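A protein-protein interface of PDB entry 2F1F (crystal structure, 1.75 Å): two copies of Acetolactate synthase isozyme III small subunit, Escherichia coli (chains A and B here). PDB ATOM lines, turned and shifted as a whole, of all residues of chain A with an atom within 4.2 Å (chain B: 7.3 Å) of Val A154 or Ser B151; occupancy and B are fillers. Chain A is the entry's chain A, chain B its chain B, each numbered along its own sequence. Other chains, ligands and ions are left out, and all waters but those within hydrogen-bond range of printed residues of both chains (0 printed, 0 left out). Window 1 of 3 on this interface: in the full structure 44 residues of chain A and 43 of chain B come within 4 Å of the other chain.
The guanidinium group of Arg B150 lies within salt-bridge range of the side-chain carboxylate of Glu B86. The backbone NH (N) of Thr B48 lies within hydrogen-bond range of the backbone carbonyl oxygen (O) of Thr B35, at 2.7 Å. N of Thr A48 sits at hydrogen-bond distance from O of Thr A35 (2.8 Å). The backbone carbonyl oxygen (O) of Ile B87 sits at hydrogen-bond distance from the backbone NH (N) of Ser B151 (2.8 Å). O of Arg A85 lies within hydrogen-bond range of N of Val A154 (2.7 Å). N of Ala B149 is in hydrogen-bond range of O of Leu B89, 2.8 Å away.
Thr A35 touches Leu B34. Thr A35 touches Ser B151. Ser B33 touches Val A36. CG2 of Val A83 touches CD1 of Leu B89 (3.97 Å). Thr B35 touches Ser A151 (CB to O, 3.6 Å). CG1 of Val B154 touches CA of Ser A151, 3.6 Å away. Val A154 touches Leu B89 (O to CD1, 3.95 Å). Val A154 touches Arg B150. CG1 of Val A154 touches CA of Ser B151, 3.5 Å away. Gly A155 touches Ala B149.
N of Val A36 lies within hydrogen-bond range of O of Leu B34 (2.9 Å).
Printed residues of chain B within 4 Å of Val A154: Leu B89, Arg B150 and Ser B151. Printed residues of chain A within 4 Å of Ser B151: Thr A35 (3.5 Å), Ser A151 (3.98 Å) and Val A154 (3.5 Å). Printed residues of chain A within 4 Å of Ile B87: Arg A85. Of the printed residues of chain B, Arg A85 touches Ile B87. Printed residues of chain A within 4 Å of Val B36: Ser A151. Of the printed residues of chain A, Leu B89 touches Val A83 and Val A154. Glu B86 touches none of the printed residues of chain A. Thr A48 touches none of the printed residues of chain B. The nearest printed residue of chain A that does not touch Ser B151 is Val A36 (4.01 Å). The nearest printed residue of chain B that does not touch Ser A151 is Ile B87 (4.5 Å).
Thr A35 touches Ser B151, and with the chains exchanged Ser A151 touches Thr B35. Ser A151 touches Val B36, but with the chains exchanged Val A36 does not touch Ser B151 (4.01 Å). Ser B151 touches its own counterpart, Ser A151. Ser A151 touches Val B154, and with the chains exchanged Val A154 touches Ser B151.
Printed residues of chain B that touch a printed residue of chain A: Ser B33, Leu B34, Thr B35, Val B36, Ile B87, Leu B89, Ala B149, Arg B150, Ser B151 and Val B154. Of the 11 printed residues of chain A, 7 touch a printed residue of chain B. Printed residues of chain A that touch a printed residue of chain B: Thr A35, Val A36, Val A83, Arg A85, Ser A151, Val A154 and Gly A155. Along chain A the printed residues that touch a printed residue of chain B span positions 35 to 155. Among the printed residues, 14 pairs touch across the chains. Among the printed residues, no Asp or Glu carboxylate lies within 4 Å of a Lys or Arg side-chain nitrogen of the other chain.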
ATOM      1  N   THR A  35      -6.906 -15.812 -14.909  1.00  0.00           N
ATOM      2  CA  THR A  35      -7.137 -17.179 -15.413  1.00  0.00           C
ATOM      3  C   THR A  35      -7.852 -17.926 -14.327  1.00  0.00           C
ATOM      4  O   THR A  35      -7.537 -17.797 -13.116  1.00  0.00           O
ATOM      5  CB  THR A  35      -5.780 -17.934 -15.742  1.00  0.00           C
ATOM      6  OG1 THR A  35      -4.906 -17.946 -14.568  1.00  0.00           O
ATOM      7  CG2 THR A  35      -5.089 -17.276 -16.940  1.00  0.00           C
ATOM      8  N   VAL A  36      -8.757 -18.784 -14.735  1.00  0.00           N
ATOM      9  CA  VAL A  36      -9.496 -19.632 -13.806  1.00  0.00           C
ATOM     10  C   VAL A  36      -9.928 -20.886 -14.500  1.00  0.00           C
ATOM     11  O   VAL A  36     -10.436 -20.810 -15.606  1.00  0.00           O
ATOM     12  CB  VAL A  36     -10.684 -18.904 -13.117  1.00  0.00           C
ATOM     13  CG1 VAL A  36     -11.697 -18.374 -14.110  1.00  0.00           C
ATOM     14  CG2 VAL A  36     -11.342 -19.835 -12.096  1.00  0.00           C
ATOM     15  N   THR A  48      -5.870 -17.233 -10.931  1.00  0.00           N
ATOM     16  CA  THR A  48      -4.708 -16.375 -10.756  1.00  0.00           C
ATOM     17  C   THR A  48      -5.096 -15.008 -11.276  1.00  0.00           C
ATOM     18  O   THR A  48      -5.527 -14.864 -12.433  1.00  0.00           O
ATOM     19  CB  THR A  48      -3.398 -16.896 -11.542  1.00  0.00           C
ATOM     20  OG1 THR A  48      -3.152 -18.261 -11.222  1.00  0.00           O
ATOM     21  CG2 THR A  48      -2.236 -16.002 -11.127  1.00  0.00           C
ATOM     22  N   VAL A  83       6.493 -19.186  -9.320  1.00  0.00           N
ATOM     23  CA  VAL A  83       6.668 -19.331 -10.786  1.00  0.00           C
ATOM     24  C   VAL A  83       5.436 -18.822 -11.444  1.00  0.00           C
ATOM     25  O   VAL A  83       4.302 -19.062 -10.931  1.00  0.00           O
ATOM     26  CB  VAL A  83       6.929 -20.794 -11.242  1.00  0.00           C
ATOM     27  CG1 VAL A  83       8.169 -21.260 -10.719  1.00  0.00           C
ATOM     28  CG2 VAL A  83       5.885 -21.734 -10.780  1.00  0.00           C
ATOM     29  N   GLU A  84       5.611 -18.143 -12.553  1.00  0.00           N
ATOM     30  CA  GLU A  84       4.491 -17.630 -13.357  1.00  0.00           C
ATOM     31  C   GLU A  84       4.719 -17.979 -14.824  1.00  0.00           C
ATOM     32  O   GLU A  84       5.866 -17.928 -15.316  1.00  0.00           O
ATOM     33  CB  GLU A  84       4.201 -16.127 -13.208  1.00  0.00           C
ATOM     34  CG  GLU A  84       5.083 -15.231 -12.637  1.00  0.00           C
ATOM     35  CD  GLU A  84       4.546 -13.755 -12.667  1.00  0.00           C
ATOM     36  OE1 GLU A  84       4.447 -13.115 -11.591  1.00  0.00           O
ATOM     37  OE2 GLU A  84       4.281 -13.217 -13.762  1.00  0.00           O
ATOM     38  N   ARG A  85       3.676 -18.447 -15.470  1.00  0.00           N
ATOM     39  CA  ARG A  85       3.720 -18.775 -16.886  1.00  0.00           C
ATOM     40  C   ARG A  85       2.436 -18.302 -17.635  1.00  0.00           C
ATOM     41  O   ARG A  85       1.353 -18.096 -17.021  1.00  0.00           O
ATOM     42  CB  ARG A  85       3.901 -20.289 -17.048  1.00  0.00           C
ATOM     43  CG  ARG A  85       5.173 -20.874 -16.519  1.00  0.00           C
ATOM     44  CD  ARG A  85       6.432 -20.505 -17.379  1.00  0.00           C
ATOM     45  NE  ARG A  85       7.625 -21.258 -17.009  1.00  0.00           N
ATOM     46  CZ  ARG A  85       8.491 -20.827 -16.121  1.00  0.00           C
ATOM     47  NH1 ARG A  85       8.244 -19.690 -15.504  1.00  0.00           N
ATOM     48  NH2 ARG A  85       9.561 -21.531 -15.823  1.00  0.00           N
ATOM     49  N   SER A 151      -3.090 -16.250 -22.904  1.00  0.00           N
ATOM     50  CA  SER A 151      -3.811 -16.644 -21.740  1.00  0.00           C
ATOM     51  C   SER A 151      -3.796 -15.629 -20.596  1.00  0.00           C
ATOM     52  O   SER A 151      -4.697 -15.609 -19.724  1.00  0.00           O
ATOM     53  CB  SER A 151      -3.324 -17.998 -21.210  1.00  0.00           C
ATOM     54  OG  SER A 151      -2.010 -17.923 -20.672  1.00  0.00           O
ATOM     55  N   GLY A 152      -2.780 -14.813 -20.486  1.00  0.00           N
ATOM     56  CA  GLY A 152      -2.662 -14.279 -19.113  1.00  0.00           C
ATOM     57  C   GLY A 152      -1.994 -15.286 -18.107  1.00  0.00           C
ATOM     58  O   GLY A 152      -1.899 -16.504 -18.370  1.00  0.00           O
ATOM     59  N   VAL A 153      -1.562 -14.750 -16.966  1.00  0.00           N
ATOM     60  CA  VAL A 153      -0.650 -15.423 -16.041  1.00  0.00           C
ATOM     61  C   VAL A 153      -1.306 -16.568 -15.257  1.00  0.00           C
ATOM     62  O   VAL A 153      -2.426 -16.401 -14.779  1.00  0.00           O
ATOM     63  CB  VAL A 153       0.007 -14.432 -14.937  1.00  0.00           C
ATOM     64  CG1 VAL A 153      -0.917 -13.928 -13.978  1.00  0.00           C
ATOM     65  CG2 VAL A 153       0.913 -15.153 -14.181  1.00  0.00           C
ATOM     66  N   VAL A 154      -0.632 -17.715 -15.192  1.00  0.00           N
ATOM     67  CA  VAL A 154      -0.890 -18.805 -14.181  1.00  0.00           C
ATOM     68  C   VAL A 154       0.282 -18.858 -13.257  1.00  0.00           C
ATOM     69  O   VAL A 154       1.448 -18.659 -13.698  1.00  0.00           O
ATOM     70  CB  VAL A 154      -1.206 -20.275 -14.783  1.00  0.00           C
ATOM     71  CG1 VAL A 154      -2.310 -20.151 -15.840  1.00  0.00           C
ATOM     72  CG2 VAL A 154      -0.048 -20.823 -15.460  1.00  0.00           C
ATOM     73  N   GLY A 155       0.014 -19.019 -11.965  1.00  0.00           N
ATOM     74  CA  GLY A 155       1.075 -19.018 -10.961  1.00  0.00           C
ATOM     75  C   GLY A 155       0.946 -20.055  -9.878  1.00  0.00           C
ATOM     76  O   GLY A 155      -0.174 -20.441  -9.510  1.00  0.00           O
ATOM     77  N   SER B  33     -14.107 -22.527 -17.725  1.00  0.00           N
ATOM     78  CA  SER B  33     -12.836 -21.781 -17.639  1.00  0.00           C
ATOM     79  C   SER B  33     -12.999 -20.374 -18.209  1.00  0.00           C
ATOM     80  O   SER B  33     -13.857 -20.106 -19.078  1.00  0.00           O
ATOM     81  CB  SER B  33     -11.666 -22.564 -18.316  1.00  0.00           C
ATOM     82  OG  SER B  33     -11.659 -22.453 -19.772  1.00  0.00           O
ATOM     83  N   LEU B  34     -12.140 -19.481 -17.767  1.00  0.00           N
ATOM     84  CA  LEU B  34     -12.099 -18.124 -18.250  1.00  0.00           C
ATOM     85  C   LEU B  34     -10.649 -17.621 -18.242  1.00  0.00           C
ATOM     86  O   LEU B  34      -9.945 -17.820 -17.229  1.00  0.00           O
ATOM     87  CB  LEU B  34     -12.936 -17.254 -17.335  1.00  0.00           C
ATOM     88  CG  LEU B  34     -12.934 -15.754 -17.639  1.00  0.00           C
ATOM     89  CD1 LEU B  34     -13.603 -15.510 -18.982  1.00  0.00           C
ATOM     90  CD2 LEU B  34     -13.686 -14.972 -16.565  1.00  0.00           C
ATOM     91  N   THR B  35     -10.210 -17.063 -19.377  1.00  0.00           N
ATOM     92  CA  THR B  35      -8.955 -16.310 -19.461  1.00  0.00           C
ATOM     93  C   THR B  35      -9.205 -14.908 -19.969  1.00  0.00           C
ATOM     94  O   THR B  35      -9.999 -14.684 -20.928  1.00  0.00           O
ATOM     95  CB  THR B  35      -7.871 -17.050 -20.411  1.00  0.00           C
ATOM     96  OG1 THR B  35      -8.256 -16.923 -21.785  1.00  0.00           O
ATOM     97  CG2 THR B  35      -7.883 -18.443 -20.202  1.00  0.00           C
ATOM     98  N   VAL B  36      -8.508 -13.954 -19.365  1.00  0.00           N
ATOM     99  CA  VAL B  36      -8.516 -12.565 -19.846  1.00  0.00           C
ATOM    100  C   VAL B  36      -7.098 -11.981 -19.790  1.00  0.00           C
ATOM    101  O   VAL B  36      -6.378 -12.156 -18.785  1.00  0.00           O
ATOM    102  CB  VAL B  36      -9.679 -11.709 -19.242  1.00  0.00           C
ATOM    103  CG1 VAL B  36     -10.207 -12.216 -17.985  1.00  0.00           C
ATOM    104  CG2 VAL B  36      -9.409 -10.223 -19.222  1.00  0.00           C
ATOM    105  N   THR B  48     -11.382 -15.225 -23.240  1.00  0.00           N
ATOM    106  CA  THR B  48     -11.877 -16.506 -23.838  1.00  0.00           C
ATOM    107  C   THR B  48     -12.606 -17.288 -22.753  1.00  0.00           C
ATOM    108  O   THR B  48     -12.069 -17.526 -21.662  1.00  0.00           O
ATOM    109  CB  THR B  48     -10.731 -17.334 -24.441  1.00  0.00           C
ATOM    110  OG1 THR B  48     -10.019 -16.507 -25.360  1.00  0.00           O
ATOM    111  CG2 THR B  48     -11.268 -18.595 -25.188  1.00  0.00           C
ATOM    112  N   ARG B  85      -5.594 -24.323 -27.213  1.00  0.00           N
ATOM    113  CA  ARG B  85      -4.511 -24.796 -26.327  1.00  0.00           C
ATOM    114  C   ARG B  85      -4.674 -24.206 -24.932  1.00  0.00           C
ATOM    115  O   ARG B  85      -5.419 -23.228 -24.691  1.00  0.00           O
ATOM    116  CB  ARG B  85      -3.124 -24.417 -26.898  1.00  0.00           C
ATOM    117  CG  ARG B  85      -2.769 -25.066 -28.329  1.00  0.00           C
ATOM    118  CD  ARG B  85      -2.779 -26.556 -28.288  1.00  0.00           C
ATOM    119  NE  ARG B  85      -2.843 -27.274 -29.629  1.00  0.00           N
ATOM    120  CZ  ARG B  85      -1.728 -27.715 -30.121  1.00  0.00           C
ATOM    121  NH1 ARG B  85      -0.679 -27.504 -29.364  1.00  0.00           N
ATOM    122  NH2 ARG B  85      -1.624 -28.355 -31.240  1.00  0.00           N
ATOM    123  N   GLU B  86      -4.028 -24.854 -23.994  1.00  0.00           N
ATOM    124  CA  GLU B  86      -4.057 -24.495 -22.622  1.00  0.00           C
ATOM    125  C   GLU B  86      -2.672 -24.791 -22.001  1.00  0.00           C
ATOM    126  O   GLU B  86      -1.908 -25.611 -22.518  1.00  0.00           O
ATOM    127  CB  GLU B  86      -5.136 -25.386 -21.992  1.00  0.00           C
ATOM    128  CG  GLU B  86      -5.463 -25.148 -20.587  1.00  0.00           C
ATOM    129  CD  GLU B  86      -6.855 -25.769 -20.175  1.00  0.00           C
ATOM    130  OE1 GLU B  86      -7.495 -26.637 -20.905  1.00  0.00           O
ATOM    131  OE2 GLU B  86      -7.236 -25.389 -19.083  1.00  0.00           O
ATOM    132  N   ILE B  87      -2.364 -24.134 -20.900  1.00  0.00           N
ATOM    133  CA  ILE B  87      -1.170 -24.455 -20.078  1.00  0.00           C
ATOM    134  C   ILE B  87      -1.588 -24.779 -18.623  1.00  0.00           C
ATOM    135  O   ILE B  87      -2.537 -24.147 -18.077  1.00  0.00           O
ATOM    136  CB  ILE B  87      -0.108 -23.324 -20.126  1.00  0.00           C
ATOM    137  CG1 ILE B  87       1.228 -23.730 -19.452  1.00  0.00           C
ATOM    138  CG2 ILE B  87      -0.645 -22.002 -19.492  1.00  0.00           C
ATOM    139  CD1 ILE B  87       2.306 -22.757 -19.697  1.00  0.00           C
ATOM    140  N   MET B  88      -0.864 -25.705 -17.998  1.00  0.00           N
ATOM    141  CA  MET B  88      -1.071 -26.052 -16.622  1.00  0.00           C
ATOM    142  C   MET B  88       0.262 -26.168 -15.906  1.00  0.00           C
ATOM    143  O   MET B  88       1.229 -26.707 -16.473  1.00  0.00           O
ATOM    144  CB  MET B  88      -1.789 -27.435 -16.597  1.00  0.00           C
ATOM    145  CG  MET B  88      -1.942 -28.278 -15.417  1.00  0.00           C
ATOM    146  SD  MET B  88      -3.048 -29.726 -15.689  1.00  0.00           S
ATOM    147  CE  MET B  88      -1.985 -30.864 -16.485  1.00  0.00           C
ATOM    148  N   LEU B  89       0.233 -25.762 -14.642  1.00  0.00           N
ATOM    149  CA  LEU B  89       1.262 -26.016 -13.657  1.00  0.00           C
ATOM    150  C   LEU B  89       0.689 -26.966 -12.644  1.00  0.00           C
ATOM    151  O   LEU B  89      -0.344 -26.685 -12.048  1.00  0.00           O
ATOM    152  CB  LEU B  89       1.752 -24.755 -12.949  1.00  0.00           C
ATOM    153  CG  LEU B  89       2.263 -23.599 -13.848  1.00  0.00           C
ATOM    154  CD1 LEU B  89       2.690 -22.354 -13.050  1.00  0.00           C
ATOM    155  CD2 LEU B  89       3.306 -24.093 -14.900  1.00  0.00           C
ATOM    156  N   LEU B 125       2.917 -28.195 -18.382  1.00  0.00           N
ATOM    157  CA  LEU B 125       2.444 -28.897 -19.589  1.00  0.00           C
ATOM    158  C   LEU B 125       1.498 -28.001 -20.422  1.00  0.00           C
ATOM    159  O   LEU B 125       0.547 -27.414 -19.865  1.00  0.00           O
ATOM    160  CB  LEU B 125       1.736 -30.181 -19.182  1.00  0.00           C
ATOM    161  CG  LEU B 125       1.163 -31.056 -20.332  1.00  0.00           C
ATOM    162  CD1 LEU B 125       2.336 -31.564 -21.181  1.00  0.00           C
ATOM    163  CD2 LEU B 125       0.296 -32.196 -19.721  1.00  0.00           C
ATOM    164  N   LEU B 132      -4.046 -32.276 -21.453  1.00  0.00           N
ATOM    165  CA  LEU B 132      -3.882 -31.984 -20.037  1.00  0.00           C
ATOM    166  C   LEU B 132      -4.710 -32.911 -19.157  1.00  0.00           C
ATOM    167  O   LEU B 132      -4.255 -33.427 -18.128  1.00  0.00           O
ATOM    168  CB  LEU B 132      -4.194 -30.509 -19.768  1.00  0.00           C
ATOM    169  CG  LEU B 132      -3.116 -29.478 -20.059  1.00  0.00           C
ATOM    170  CD1 LEU B 132      -2.443 -29.609 -21.412  1.00  0.00           C
ATOM    171  CD2 LEU B 132      -3.640 -28.074 -19.837  1.00  0.00           C
ATOM    172  N   ALA B 149      -2.666 -25.361 -11.231  1.00  0.00           N
ATOM    173  CA  ALA B 149      -3.054 -24.058 -11.772  1.00  0.00           C
ATOM    174  C   ALA B 149      -3.163 -24.186 -13.302  1.00  0.00           C
ATOM    175  O   ALA B 149      -2.143 -24.338 -13.997  1.00  0.00           O
ATOM    176  CB  ALA B 149      -2.113 -22.916 -11.301  1.00  0.00           C
ATOM    177  N   ARG B 150      -4.385 -24.226 -13.816  1.00  0.00           N
ATOM    178  CA  ARG B 150      -4.621 -24.342 -15.270  1.00  0.00           C
ATOM    179  C   ARG B 150      -5.087 -23.020 -15.877  1.00  0.00           C
ATOM    180  O   ARG B 150      -5.874 -22.294 -15.267  1.00  0.00           O
ATOM    181  CB  ARG B 150      -5.724 -25.397 -15.620  1.00  0.00           C
ATOM    182  CG  ARG B 150      -5.440 -26.740 -15.780  1.00  0.00           C
ATOM    183  CD  ARG B 150      -6.759 -27.431 -16.178  1.00  0.00           C
ATOM    184  NE  ARG B 150      -7.027 -27.739 -17.587  1.00  0.00           N
ATOM    185  CZ  ARG B 150      -7.339 -28.956 -18.036  1.00  0.00           C
ATOM    186  NH1 ARG B 150      -7.391 -29.961 -17.181  1.00  0.00           N
ATOM    187  NH2 ARG B 150      -7.600 -29.171 -19.316  1.00  0.00           N
ATOM    188  N   SER B 151      -4.707 -22.712 -17.106  1.00  0.00           N
ATOM    189  CA  SER B 151      -5.038 -21.414 -17.679  1.00  0.00           C
ATOM    190  C   SER B 151      -6.511 -21.264 -18.094  1.00  0.00           C
ATOM    191  O   SER B 151      -7.039 -20.135 -18.094  1.00  0.00           O
ATOM    192  CB  SER B 151      -4.153 -21.122 -18.893  1.00  0.00           C
ATOM    193  OG  SER B 151      -4.348 -22.063 -19.960  1.00  0.00           O
ATOM    194  N   GLY B 152      -7.152 -22.336 -18.537  1.00  0.00           N
ATOM    195  CA  GLY B 152      -8.262 -22.168 -19.437  1.00  0.00           C
ATOM    196  C   GLY B 152      -7.804 -22.148 -20.918  1.00  0.00           C
ATOM    197  O   GLY B 152      -6.644 -21.865 -21.229  1.00  0.00           O
ATOM    198  N   VAL B 153      -8.700 -22.499 -21.817  1.00  0.00           N
ATOM    199  CA  VAL B 153      -8.345 -22.489 -23.242  1.00  0.00           C
ATOM    200  C   VAL B 153      -8.195 -21.113 -23.849  1.00  0.00           C
ATOM    201  O   VAL B 153      -8.908 -20.116 -23.459  1.00  0.00           O
ATOM    202  CB  VAL B 153      -9.296 -23.309 -24.138  1.00  0.00           C
ATOM    203  CG1 VAL B 153      -9.079 -24.763 -23.892  1.00  0.00           C
ATOM    204  CG2 VAL B 153     -10.685 -22.909 -23.917  1.00  0.00           C
ATOM    205  N   VAL B 154      -7.242 -21.032 -24.767  1.00  0.00           N
ATOM    206  CA  VAL B 154      -7.133 -19.960 -25.769  1.00  0.00           C
ATOM    207  C   VAL B 154      -7.189 -20.570 -27.176  1.00  0.00           C
ATOM    208  O   VAL B 154      -6.920 -21.766 -27.350  1.00  0.00           O
ATOM    209  CB  VAL B 154      -5.890 -19.065 -25.571  1.00  0.00           C
ATOM    210  CG1 VAL B 154      -5.853 -18.401 -24.154  1.00  0.00           C
ATOM    211  CG2 VAL B 154      -4.642 -19.811 -25.876  1.00  0.00           C
